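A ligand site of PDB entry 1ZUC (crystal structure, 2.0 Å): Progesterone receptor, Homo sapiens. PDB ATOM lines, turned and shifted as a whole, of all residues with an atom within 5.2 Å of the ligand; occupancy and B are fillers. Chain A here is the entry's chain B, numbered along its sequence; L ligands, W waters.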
ATOM      1  N   LEU A  41      14.153 -20.295  -5.123  1.00  0.00           N
ATOM      2  CA  LEU A  41      13.723 -21.147  -6.259  1.00  0.00           C
ATOM      3  C   LEU A  41      14.643 -22.363  -6.431  1.00  0.00           C
ATOM      4  O   LEU A  41      14.187 -23.498  -6.698  1.00  0.00           O
ATOM      5  CB  LEU A  41      13.580 -20.301  -7.554  1.00  0.00           C
ATOM      6  CG  LEU A  41      12.461 -19.230  -7.526  1.00  0.00           C
ATOM      7  CD1 LEU A  41      12.485 -18.344  -8.774  1.00  0.00           C
ATOM      8  CD2 LEU A  41      11.061 -19.890  -7.362  1.00  0.00           C
ATOM      9  N   LEU A  44      13.584 -24.728  -3.749  1.00  0.00           N
ATOM     10  CA  LEU A  44      12.302 -25.329  -4.149  1.00  0.00           C
ATOM     11  C   LEU A  44      12.506 -26.448  -5.182  1.00  0.00           C
ATOM     12  O   LEU A  44      11.849 -27.515  -5.136  1.00  0.00           O
ATOM     13  CB  LEU A  44      11.310 -24.264  -4.662  1.00  0.00           C
ATOM     14  CG  LEU A  44      10.618 -23.459  -3.541  1.00  0.00           C
ATOM     15  CD1 LEU A  44       9.854 -22.234  -4.112  1.00  0.00           C
ATOM     16  CD2 LEU A  44       9.658 -24.386  -2.733  1.00  0.00           C
ATOM     17  N   ASN A  45      13.426 -26.204  -6.113  1.00  0.00           N
ATOM     18  CA  ASN A  45      13.814 -27.236  -7.100  1.00  0.00           C
ATOM     19  C   ASN A  45      14.603 -28.403  -6.513  1.00  0.00           C
ATOM     20  O   ASN A  45      14.425 -29.548  -6.922  1.00  0.00           O
ATOM     21  CB  ASN A  45      14.567 -26.608  -8.284  1.00  0.00           C
ATOM     22  CG  ASN A  45      13.663 -25.771  -9.172  1.00  0.00           C
ATOM     23  OD1 ASN A  45      12.443 -25.970  -9.237  1.00  0.00           O
ATOM     24  ND2 ASN A  45      14.265 -24.838  -9.896  1.00  0.00           N
ATOM     25  N   LEU A  47      14.296 -29.404  -3.265  1.00  0.00           N
ATOM     26  CA  LEU A  47      13.183 -30.061  -2.609  1.00  0.00           C
ATOM     27  C   LEU A  47      12.369 -30.878  -3.603  1.00  0.00           C
ATOM     28  O   LEU A  47      12.049 -32.037  -3.364  1.00  0.00           O
ATOM     29  CB  LEU A  47      12.273 -29.020  -1.892  1.00  0.00           C
ATOM     30  CG  LEU A  47      11.266 -29.583  -0.901  1.00  0.00           C
ATOM     31  CD1 LEU A  47      11.975 -30.441   0.184  1.00  0.00           C
ATOM     32  CD2 LEU A  47      10.354 -28.483  -0.346  1.00  0.00           C
ATOM     33  N   GLY A  48      12.021 -30.266  -4.731  1.00  0.00           N
ATOM     34  CA  GLY A  48      11.391 -30.971  -5.820  1.00  0.00           C
ATOM     35  C   GLY A  48      12.072 -32.257  -6.263  1.00  0.00           C
ATOM     36  O   GLY A  48      11.420 -33.307  -6.371  1.00  0.00           O
ATOM     37  N   GLN A  51      11.576 -34.786  -3.530  1.00  0.00           N
ATOM     38  CA  GLN A  51      10.213 -35.225  -3.569  1.00  0.00           C
ATOM     39  C   GLN A  51       9.930 -36.164  -4.739  1.00  0.00           C
ATOM     40  O   GLN A  51       9.193 -37.120  -4.607  1.00  0.00           O
ATOM     41  CB  GLN A  51       9.240 -34.060  -3.480  1.00  0.00           C
ATOM     42  CG  GLN A  51       9.226 -33.392  -2.114  1.00  0.00           C
ATOM     43  CD  GLN A  51       8.256 -32.254  -2.011  1.00  0.00           C
ATOM     44  OE1 GLN A  51       7.402 -32.091  -2.857  1.00  0.00           O
ATOM     45  NE2 GLN A  51       8.397 -31.452  -0.980  1.00  0.00           N
ATOM     46  N   TRP A  81       3.547 -34.786 -11.115  1.00  0.00           N
ATOM     47  CA  TRP A  81       4.455 -34.388 -10.039  1.00  0.00           C
ATOM     48  C   TRP A  81       4.173 -33.040  -9.386  1.00  0.00           C
ATOM     49  O   TRP A  81       4.279 -32.941  -8.166  1.00  0.00           O
ATOM     50  CB  TRP A  81       5.926 -34.460 -10.492  1.00  0.00           C
ATOM     51  CG  TRP A  81       6.261 -33.488 -11.513  1.00  0.00           C
ATOM     52  CD1 TRP A  81       6.183 -33.674 -12.848  1.00  0.00           C
ATOM     53  CD2 TRP A  81       6.787 -32.141 -11.309  1.00  0.00           C
ATOM     54  NE1 TRP A  81       6.564 -32.504 -13.505  1.00  0.00           N
ATOM     55  CE2 TRP A  81       6.954 -31.566 -12.579  1.00  0.00           C
ATOM     56  CE3 TRP A  81       7.106 -31.381 -10.176  1.00  0.00           C
ATOM     57  CZ2 TRP A  81       7.422 -30.274 -12.769  1.00  0.00           C
ATOM     58  CZ3 TRP A  81       7.567 -30.074 -10.359  1.00  0.00           C
ATOM     59  CH2 TRP A  81       7.729 -29.537 -11.654  1.00  0.00           C
ATOM     60  N   MET A  82       3.854 -32.008 -10.161  1.00  0.00           N
ATOM     61  CA  MET A  82       3.571 -30.687  -9.554  1.00  0.00           C
ATOM     62  C   MET A  82       2.312 -30.756  -8.689  1.00  0.00           C
ATOM     63  O   MET A  82       2.293 -30.221  -7.557  1.00  0.00           O
ATOM     64  CB  MET A  82       3.452 -29.571 -10.618  1.00  0.00           C
ATOM     65  CG  MET A  82       3.185 -28.183  -9.997  1.00  0.00           C
ATOM     66  SD  MET A  82       4.630 -27.497  -9.145  1.00  0.00           S
ATOM     67  CE  MET A  82       5.559 -27.005 -10.574  1.00  0.00           C
ATOM     68  N   MET A  85       3.216 -32.574  -5.440  1.00  0.00           N
ATOM     69  CA  MET A  85       3.984 -31.668  -4.566  1.00  0.00           C
ATOM     70  C   MET A  85       3.141 -30.614  -3.877  1.00  0.00           C
ATOM     71  O   MET A  85       3.261 -30.379  -2.644  1.00  0.00           O
ATOM     72  CB  MET A  85       5.118 -30.974  -5.343  1.00  0.00           C
ATOM     73  CG  MET A  85       6.229 -31.948  -5.667  1.00  0.00           C
ATOM     74  SD  MET A  85       7.523 -31.068  -6.547  1.00  0.00           S
ATOM     75  CE  MET A  85       8.343 -32.580  -7.023  1.00  0.00           C
ATOM     76  N   VAL A  86       2.279 -29.960  -4.649  1.00  0.00           N
ATOM     77  CA  VAL A  86       1.451 -28.896  -4.088  1.00  0.00           C
ATOM     78  C   VAL A  86       0.352 -29.433  -3.118  1.00  0.00           C
ATOM     79  O   VAL A  86       0.014 -28.789  -2.112  1.00  0.00           O
ATOM     80  CB  VAL A  86       0.866 -27.968  -5.189  1.00  0.00           C
ATOM     81  CG1 VAL A  86      -0.356 -28.588  -5.835  1.00  0.00           C
ATOM     82  CG2 VAL A  86       0.578 -26.588  -4.641  1.00  0.00           C
ATOM     83  N   LEU A  89       2.260 -30.234   0.046  1.00  0.00           N
ATOM     84  CA  LEU A  89       2.500 -28.946   0.719  1.00  0.00           C
ATOM     85  C   LEU A  89       1.272 -28.483   1.500  1.00  0.00           C
ATOM     86  O   LEU A  89       1.385 -28.014   2.658  1.00  0.00           O
ATOM     87  CB  LEU A  89       2.862 -27.879  -0.322  1.00  0.00           C
ATOM     88  CG  LEU A  89       2.839 -26.407   0.064  1.00  0.00           C
ATOM     89  CD1 LEU A  89       3.943 -26.095   1.121  1.00  0.00           C
ATOM     90  CD2 LEU A  89       2.988 -25.560  -1.210  1.00  0.00           C
ATOM     91  N   ARG A  92       0.990 -30.864   4.788  1.00  0.00           N
ATOM     92  CA  ARG A  92       1.997 -30.367   5.780  1.00  0.00           C
ATOM     93  C   ARG A  92       1.683 -28.999   6.373  1.00  0.00           C
ATOM     94  O   ARG A  92       1.777 -28.780   7.602  1.00  0.00           O
ATOM     95  CB  ARG A  92       3.407 -30.330   5.164  1.00  0.00           C
ATOM     96  CG  ARG A  92       3.941 -31.711   4.902  1.00  0.00           C
ATOM     97  CD  ARG A  92       5.430 -31.704   4.545  1.00  0.00           C
ATOM     98  NE  ARG A  92       5.705 -30.879   3.375  1.00  0.00           N
ATOM     99  CZ  ARG A  92       5.510 -31.253   2.111  1.00  0.00           C
ATOM    100  NH1 ARG A  92       4.998 -32.456   1.812  1.00  0.00           N
ATOM    101  NH2 ARG A  92       5.802 -30.408   1.137  1.00  0.00           N
ATOM    102  N   PHE A 104       6.830 -25.994   3.103  1.00  0.00           N
ATOM    103  CA  PHE A 104       7.460 -26.775   2.035  1.00  0.00           C
ATOM    104  C   PHE A 104       8.255 -27.919   2.682  1.00  0.00           C
ATOM    105  O   PHE A 104       8.151 -29.090   2.276  1.00  0.00           O
ATOM    106  CB  PHE A 104       8.379 -25.876   1.163  1.00  0.00           C
ATOM    107  CG  PHE A 104       7.638 -24.836   0.364  1.00  0.00           C
ATOM    108  CD1 PHE A 104       7.582 -23.509   0.804  1.00  0.00           C
ATOM    109  CD2 PHE A 104       7.018 -25.163  -0.834  1.00  0.00           C
ATOM    110  CE1 PHE A 104       6.918 -22.530   0.028  1.00  0.00           C
ATOM    111  CE2 PHE A 104       6.351 -24.204  -1.583  1.00  0.00           C
ATOM    112  CZ  PHE A 104       6.306 -22.889  -1.166  1.00  0.00           C
ATOM    113  N   PHE A 120       7.917 -13.780  -5.653  1.00  0.00           N
ATOM    114  CA  PHE A 120       6.786 -14.505  -6.255  1.00  0.00           C
ATOM    115  C   PHE A 120       5.592 -14.623  -5.264  1.00  0.00           C
ATOM    116  O   PHE A 120       5.023 -15.706  -5.076  1.00  0.00           O
ATOM    117  CB  PHE A 120       7.216 -15.866  -6.833  1.00  0.00           C
ATOM    118  CG  PHE A 120       8.052 -16.714  -5.892  1.00  0.00           C
ATOM    119  CD1 PHE A 120       7.485 -17.766  -5.202  1.00  0.00           C
ATOM    120  CD2 PHE A 120       9.399 -16.456  -5.722  1.00  0.00           C
ATOM    121  CE1 PHE A 120       8.263 -18.559  -4.317  1.00  0.00           C
ATOM    122  CE2 PHE A 120      10.196 -17.245  -4.874  1.00  0.00           C
ATOM    123  CZ  PHE A 120       9.645 -18.280  -4.176  1.00  0.00           C
ATOM    124  N   LEU A 123       2.230 -16.162  -6.621  1.00  0.00           N
ATOM    125  CA  LEU A 123       2.347 -17.590  -6.739  1.00  0.00           C
ATOM    126  C   LEU A 123       2.254 -18.241  -5.370  1.00  0.00           C
ATOM    127  O   LEU A 123       1.599 -19.257  -5.256  1.00  0.00           O
ATOM    128  CB  LEU A 123       3.699 -17.970  -7.352  1.00  0.00           C
ATOM    129  CG  LEU A 123       3.761 -19.306  -8.094  1.00  0.00           C
ATOM    130  CD1 LEU A 123       3.136 -19.127  -9.457  1.00  0.00           C
ATOM    131  CD2 LEU A 123       5.225 -19.735  -8.199  1.00  0.00           C
ATOM    132  N   MET A 127      -0.534 -21.062  -4.213  1.00  0.00           N
ATOM    133  CA  MET A 127      -0.240 -22.296  -3.506  1.00  0.00           C
ATOM    134  C   MET A 127      -0.966 -22.355  -2.135  1.00  0.00           C
ATOM    135  O   MET A 127      -1.533 -23.395  -1.770  1.00  0.00           O
ATOM    136  CB  MET A 127       1.277 -22.443  -3.365  1.00  0.00           C
ATOM    137  CG  MET A 127       1.988 -22.739  -4.729  1.00  0.00           C
ATOM    138  SD  MET A 127       3.751 -23.116  -4.543  1.00  0.00           S
ATOM    139  CE  MET A 127       4.516 -21.540  -4.316  1.00  0.00           C
ATOM    140  N   LEU A 213       1.267 -22.801 -11.801  1.00  0.00           N
ATOM    141  CA  LEU A 213       2.568 -23.295 -11.342  1.00  0.00           C
ATOM    142  C   LEU A 213       3.384 -23.832 -12.497  1.00  0.00           C
ATOM    143  O   LEU A 213       4.554 -23.495 -12.630  1.00  0.00           O
ATOM    144  CB  LEU A 213       2.408 -24.365 -10.257  1.00  0.00           C
ATOM    145  CG  LEU A 213       1.528 -23.957  -9.056  1.00  0.00           C
ATOM    146  CD1 LEU A 213       1.573 -25.070  -7.933  1.00  0.00           C
ATOM    147  CD2 LEU A 213       1.862 -22.593  -8.526  1.00  0.00           C
ATOM    148  N   TYR A 216       4.787 -20.889 -14.697  1.00  0.00           N
ATOM    149  CA  TYR A 216       5.856 -20.191 -13.971  1.00  0.00           C
ATOM    150  C   TYR A 216       7.151 -21.044 -13.965  1.00  0.00           C
ATOM    151  O   TYR A 216       8.280 -20.545 -14.151  1.00  0.00           O
ATOM    152  CB  TYR A 216       5.427 -19.912 -12.496  1.00  0.00           C
ATOM    153  CG  TYR A 216       6.461 -19.093 -11.712  1.00  0.00           C
ATOM    154  CD1 TYR A 216       7.592 -19.703 -11.150  1.00  0.00           C
ATOM    155  CD2 TYR A 216       6.307 -17.708 -11.563  1.00  0.00           C
ATOM    156  CE1 TYR A 216       8.533 -18.932 -10.418  1.00  0.00           C
ATOM    157  CE2 TYR A 216       7.262 -16.945 -10.847  1.00  0.00           C
ATOM    158  CZ  TYR A 216       8.362 -17.558 -10.306  1.00  0.00           C
ATOM    159  OH  TYR A 216       9.303 -16.825  -9.640  1.00  0.00           O
ATOM    160  N   CYS A 217       6.975 -22.338 -13.701  1.00  0.00           N
ATOM    161  CA  CYS A 217       8.073 -23.293 -13.661  1.00  0.00           C
ATOM    162  C   CYS A 217       8.729 -23.395 -15.041  1.00  0.00           C
ATOM    163  O   CYS A 217       9.948 -23.291 -15.184  1.00  0.00           O
ATOM    164  CB  CYS A 217       7.568 -24.678 -13.181  1.00  0.00           C
ATOM    165  SG  CYS A 217       8.887 -25.951 -13.209  1.00  0.00           S
ATOM    166  N   THR A 220      10.628 -20.193 -15.839  1.00  0.00           N
ATOM    167  CA  THR A 220      11.820 -20.132 -15.016  1.00  0.00           C
ATOM    168  C   THR A 220      12.901 -21.130 -15.539  1.00  0.00           C
ATOM    169  O   THR A 220      14.085 -20.762 -15.597  1.00  0.00           O
ATOM    170  CB  THR A 220      11.506 -20.388 -13.525  1.00  0.00           C
ATOM    171  OG1 THR A 220      10.490 -19.445 -13.089  1.00  0.00           O
ATOM    172  CG2 THR A 220      12.789 -20.303 -12.673  1.00  0.00           C
ATOM    173  N   VAL A 229      18.804 -19.986 -11.373  1.00  0.00           N
ATOM    174  CA  VAL A 229      18.009 -21.005 -10.692  1.00  0.00           C
ATOM    175  C   VAL A 229      18.487 -22.368 -11.178  1.00  0.00           C
ATOM    176  O   VAL A 229      18.446 -22.639 -12.365  1.00  0.00           O
ATOM    177  CB  VAL A 229      16.522 -20.766 -10.981  1.00  0.00           C
ATOM    178  CG1 VAL A 229      15.642 -21.905 -10.439  1.00  0.00           C
ATOM    179  CG2 VAL A 229      16.077 -19.382 -10.421  1.00  0.00           C
ATOM    180  N   PHE A 231      18.177 -26.396 -11.778  1.00  0.00           N
ATOM    181  CA  PHE A 231      17.184 -27.446 -11.895  1.00  0.00           C
ATOM    182  C   PHE A 231      17.937 -28.770 -11.906  1.00  0.00           C
ATOM    183  O   PHE A 231      18.654 -29.022 -12.868  1.00  0.00           O
ATOM    184  CB  PHE A 231      16.373 -27.297 -13.198  1.00  0.00           C
ATOM    185  CG  PHE A 231      15.335 -26.191 -13.143  1.00  0.00           C
ATOM    186  CD1 PHE A 231      15.709 -24.862 -13.335  1.00  0.00           C
ATOM    187  CD2 PHE A 231      13.983 -26.485 -12.908  1.00  0.00           C
ATOM    188  CE1 PHE A 231      14.801 -23.849 -13.300  1.00  0.00           C
ATOM    189  CE2 PHE A 231      13.047 -25.457 -12.843  1.00  0.00           C
ATOM    190  CZ  PHE A 231      13.458 -24.127 -13.079  1.00  0.00           C
ATOM    191  N   MET A 235      14.218 -33.442 -12.148  1.00  0.00           N
ATOM    192  CA  MET A 235      13.355 -32.248 -12.309  1.00  0.00           C
ATOM    193  C   MET A 235      13.461 -31.753 -13.754  1.00  0.00           C
ATOM    194  O   MET A 235      12.466 -31.593 -14.440  1.00  0.00           O
ATOM    195  CB  MET A 235      13.735 -31.114 -11.319  1.00  0.00           C
ATOM    196  CG  MET A 235      13.243 -31.277  -9.924  1.00  0.00           C
ATOM    197  SD  MET A 235      11.427 -31.079  -9.746  1.00  0.00           S
ATOM    198  CE  MET A 235      11.331 -29.334 -10.251  1.00  0.00           C
HETATM  199  C1  LIG L   1       7.893 -22.117  -7.622  1.00  0.00           C
HETATM  200  C2  LIG L   1       7.570 -23.222  -8.671  1.00  0.00           C
HETATM  201  C3  LIG L   1       7.921 -24.561  -8.056  1.00  0.00           C
HETATM  202  C4  LIG L   1       7.124 -25.206  -7.081  1.00  0.00           C
HETATM  203  C5  LIG L   1       7.498 -26.440  -6.528  1.00  0.00           C
HETATM  204  C6  LIG L   1       8.716 -27.023  -6.888  1.00  0.00           C
HETATM  205  C7  LIG L   1       9.538 -26.410  -7.843  1.00  0.00           C
HETATM  206  C8  LIG L   1       9.126 -25.195  -8.404  1.00  0.00           C
HETATM  207  N1  LIG L   1       9.969 -24.619  -9.347  1.00  0.00           N
HETATM  208  C9  LIG L   1       9.655 -23.433  -9.951  1.00  0.00           C
HETATM  209  S1  LIG L   1      10.623 -22.679 -11.025  1.00  0.00           S
HETATM  210  O1  LIG L   1       8.509 -22.782  -9.706  1.00  0.00           O
HETATM  211  C10 LIG L   1       6.636 -26.982  -5.482  1.00  0.00           C
HETATM  212  C11 LIG L   1       5.258 -26.814  -5.261  1.00  0.00           C
HETATM  213  C12 LIG L   1       4.983 -27.420  -4.008  1.00  0.00           C
HETATM  214  C13 LIG L   1       6.157 -27.912  -3.488  1.00  0.00           C
HETATM  215  N2  LIG L   1       7.184 -27.616  -4.363  1.00  0.00           N
HETATM  216  C14 LIG L   1       8.586 -27.993  -4.101  1.00  0.00           C
HETATM  217  C15 LIG L   1       6.381 -28.608  -2.287  1.00  0.00           C
HETATM  218  N3  LIG L   1       6.623 -29.162  -1.307  1.00  0.00           N
HETATM  219  C16 LIG L   1       6.158 -23.093  -9.247  1.00  0.00           C
HETATM  220  O   HOH W   1       4.871 -32.080  -1.211  1.00  0.00           O
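The side-chain amide oxygen (OD1) of Asn 45 lies within hydrogen-bond range of a nitrogen (N1) of the ligand.
A nitrogen (N3) of the ligand lies within hydrogen-bond range of the guanidinium group of Arg 92.
NE2 of Gln 51 is in hydrogen-bond range of N3 of the ligand (2.9 Å).
ND2 of Asn 45 sits close to O of Leu 41, at 3.5 Å.
The guanidinium group (NH2) of Arg 92 is in hydrogen-bond range of the backbone carbonyl oxygen (O) of Phe 104, 2.9 Å away.
The side-chain hydroxyl (OG1) of Thr 220 lies within hydrogen-bond range of the backbone carbonyl oxygen (O) of Tyr 216 (2.7 Å).
Merely in contact with the ligand: Leu 41, Leu 44, Leu 47, Met 82, Met 85, Val 86, Leu 89, Phe 104, Leu 123, Leu 213, Tyr 216, Cys 217, Thr 220 and Phe 231.
Hydrophobic or aromatic side chains that line the ligand: Leu 41, Leu 47, Met 82, Met 85, Leu 89, Phe 104, Leu 123, Tyr 216 and Phe 231.
Within 4 Å of the ligand: Leu 41, Leu 44, Asn 45, Leu 47, Gln 51, Met 82, Met 85, Val 86, Leu 89, Arg 92, Phe 104, Leu 123, Leu 213, Tyr 216, Cys 217, Thr 220 and Phe 231.
The nearest printed residue that does not touch the ligand is Met 127 (4.1 Å).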
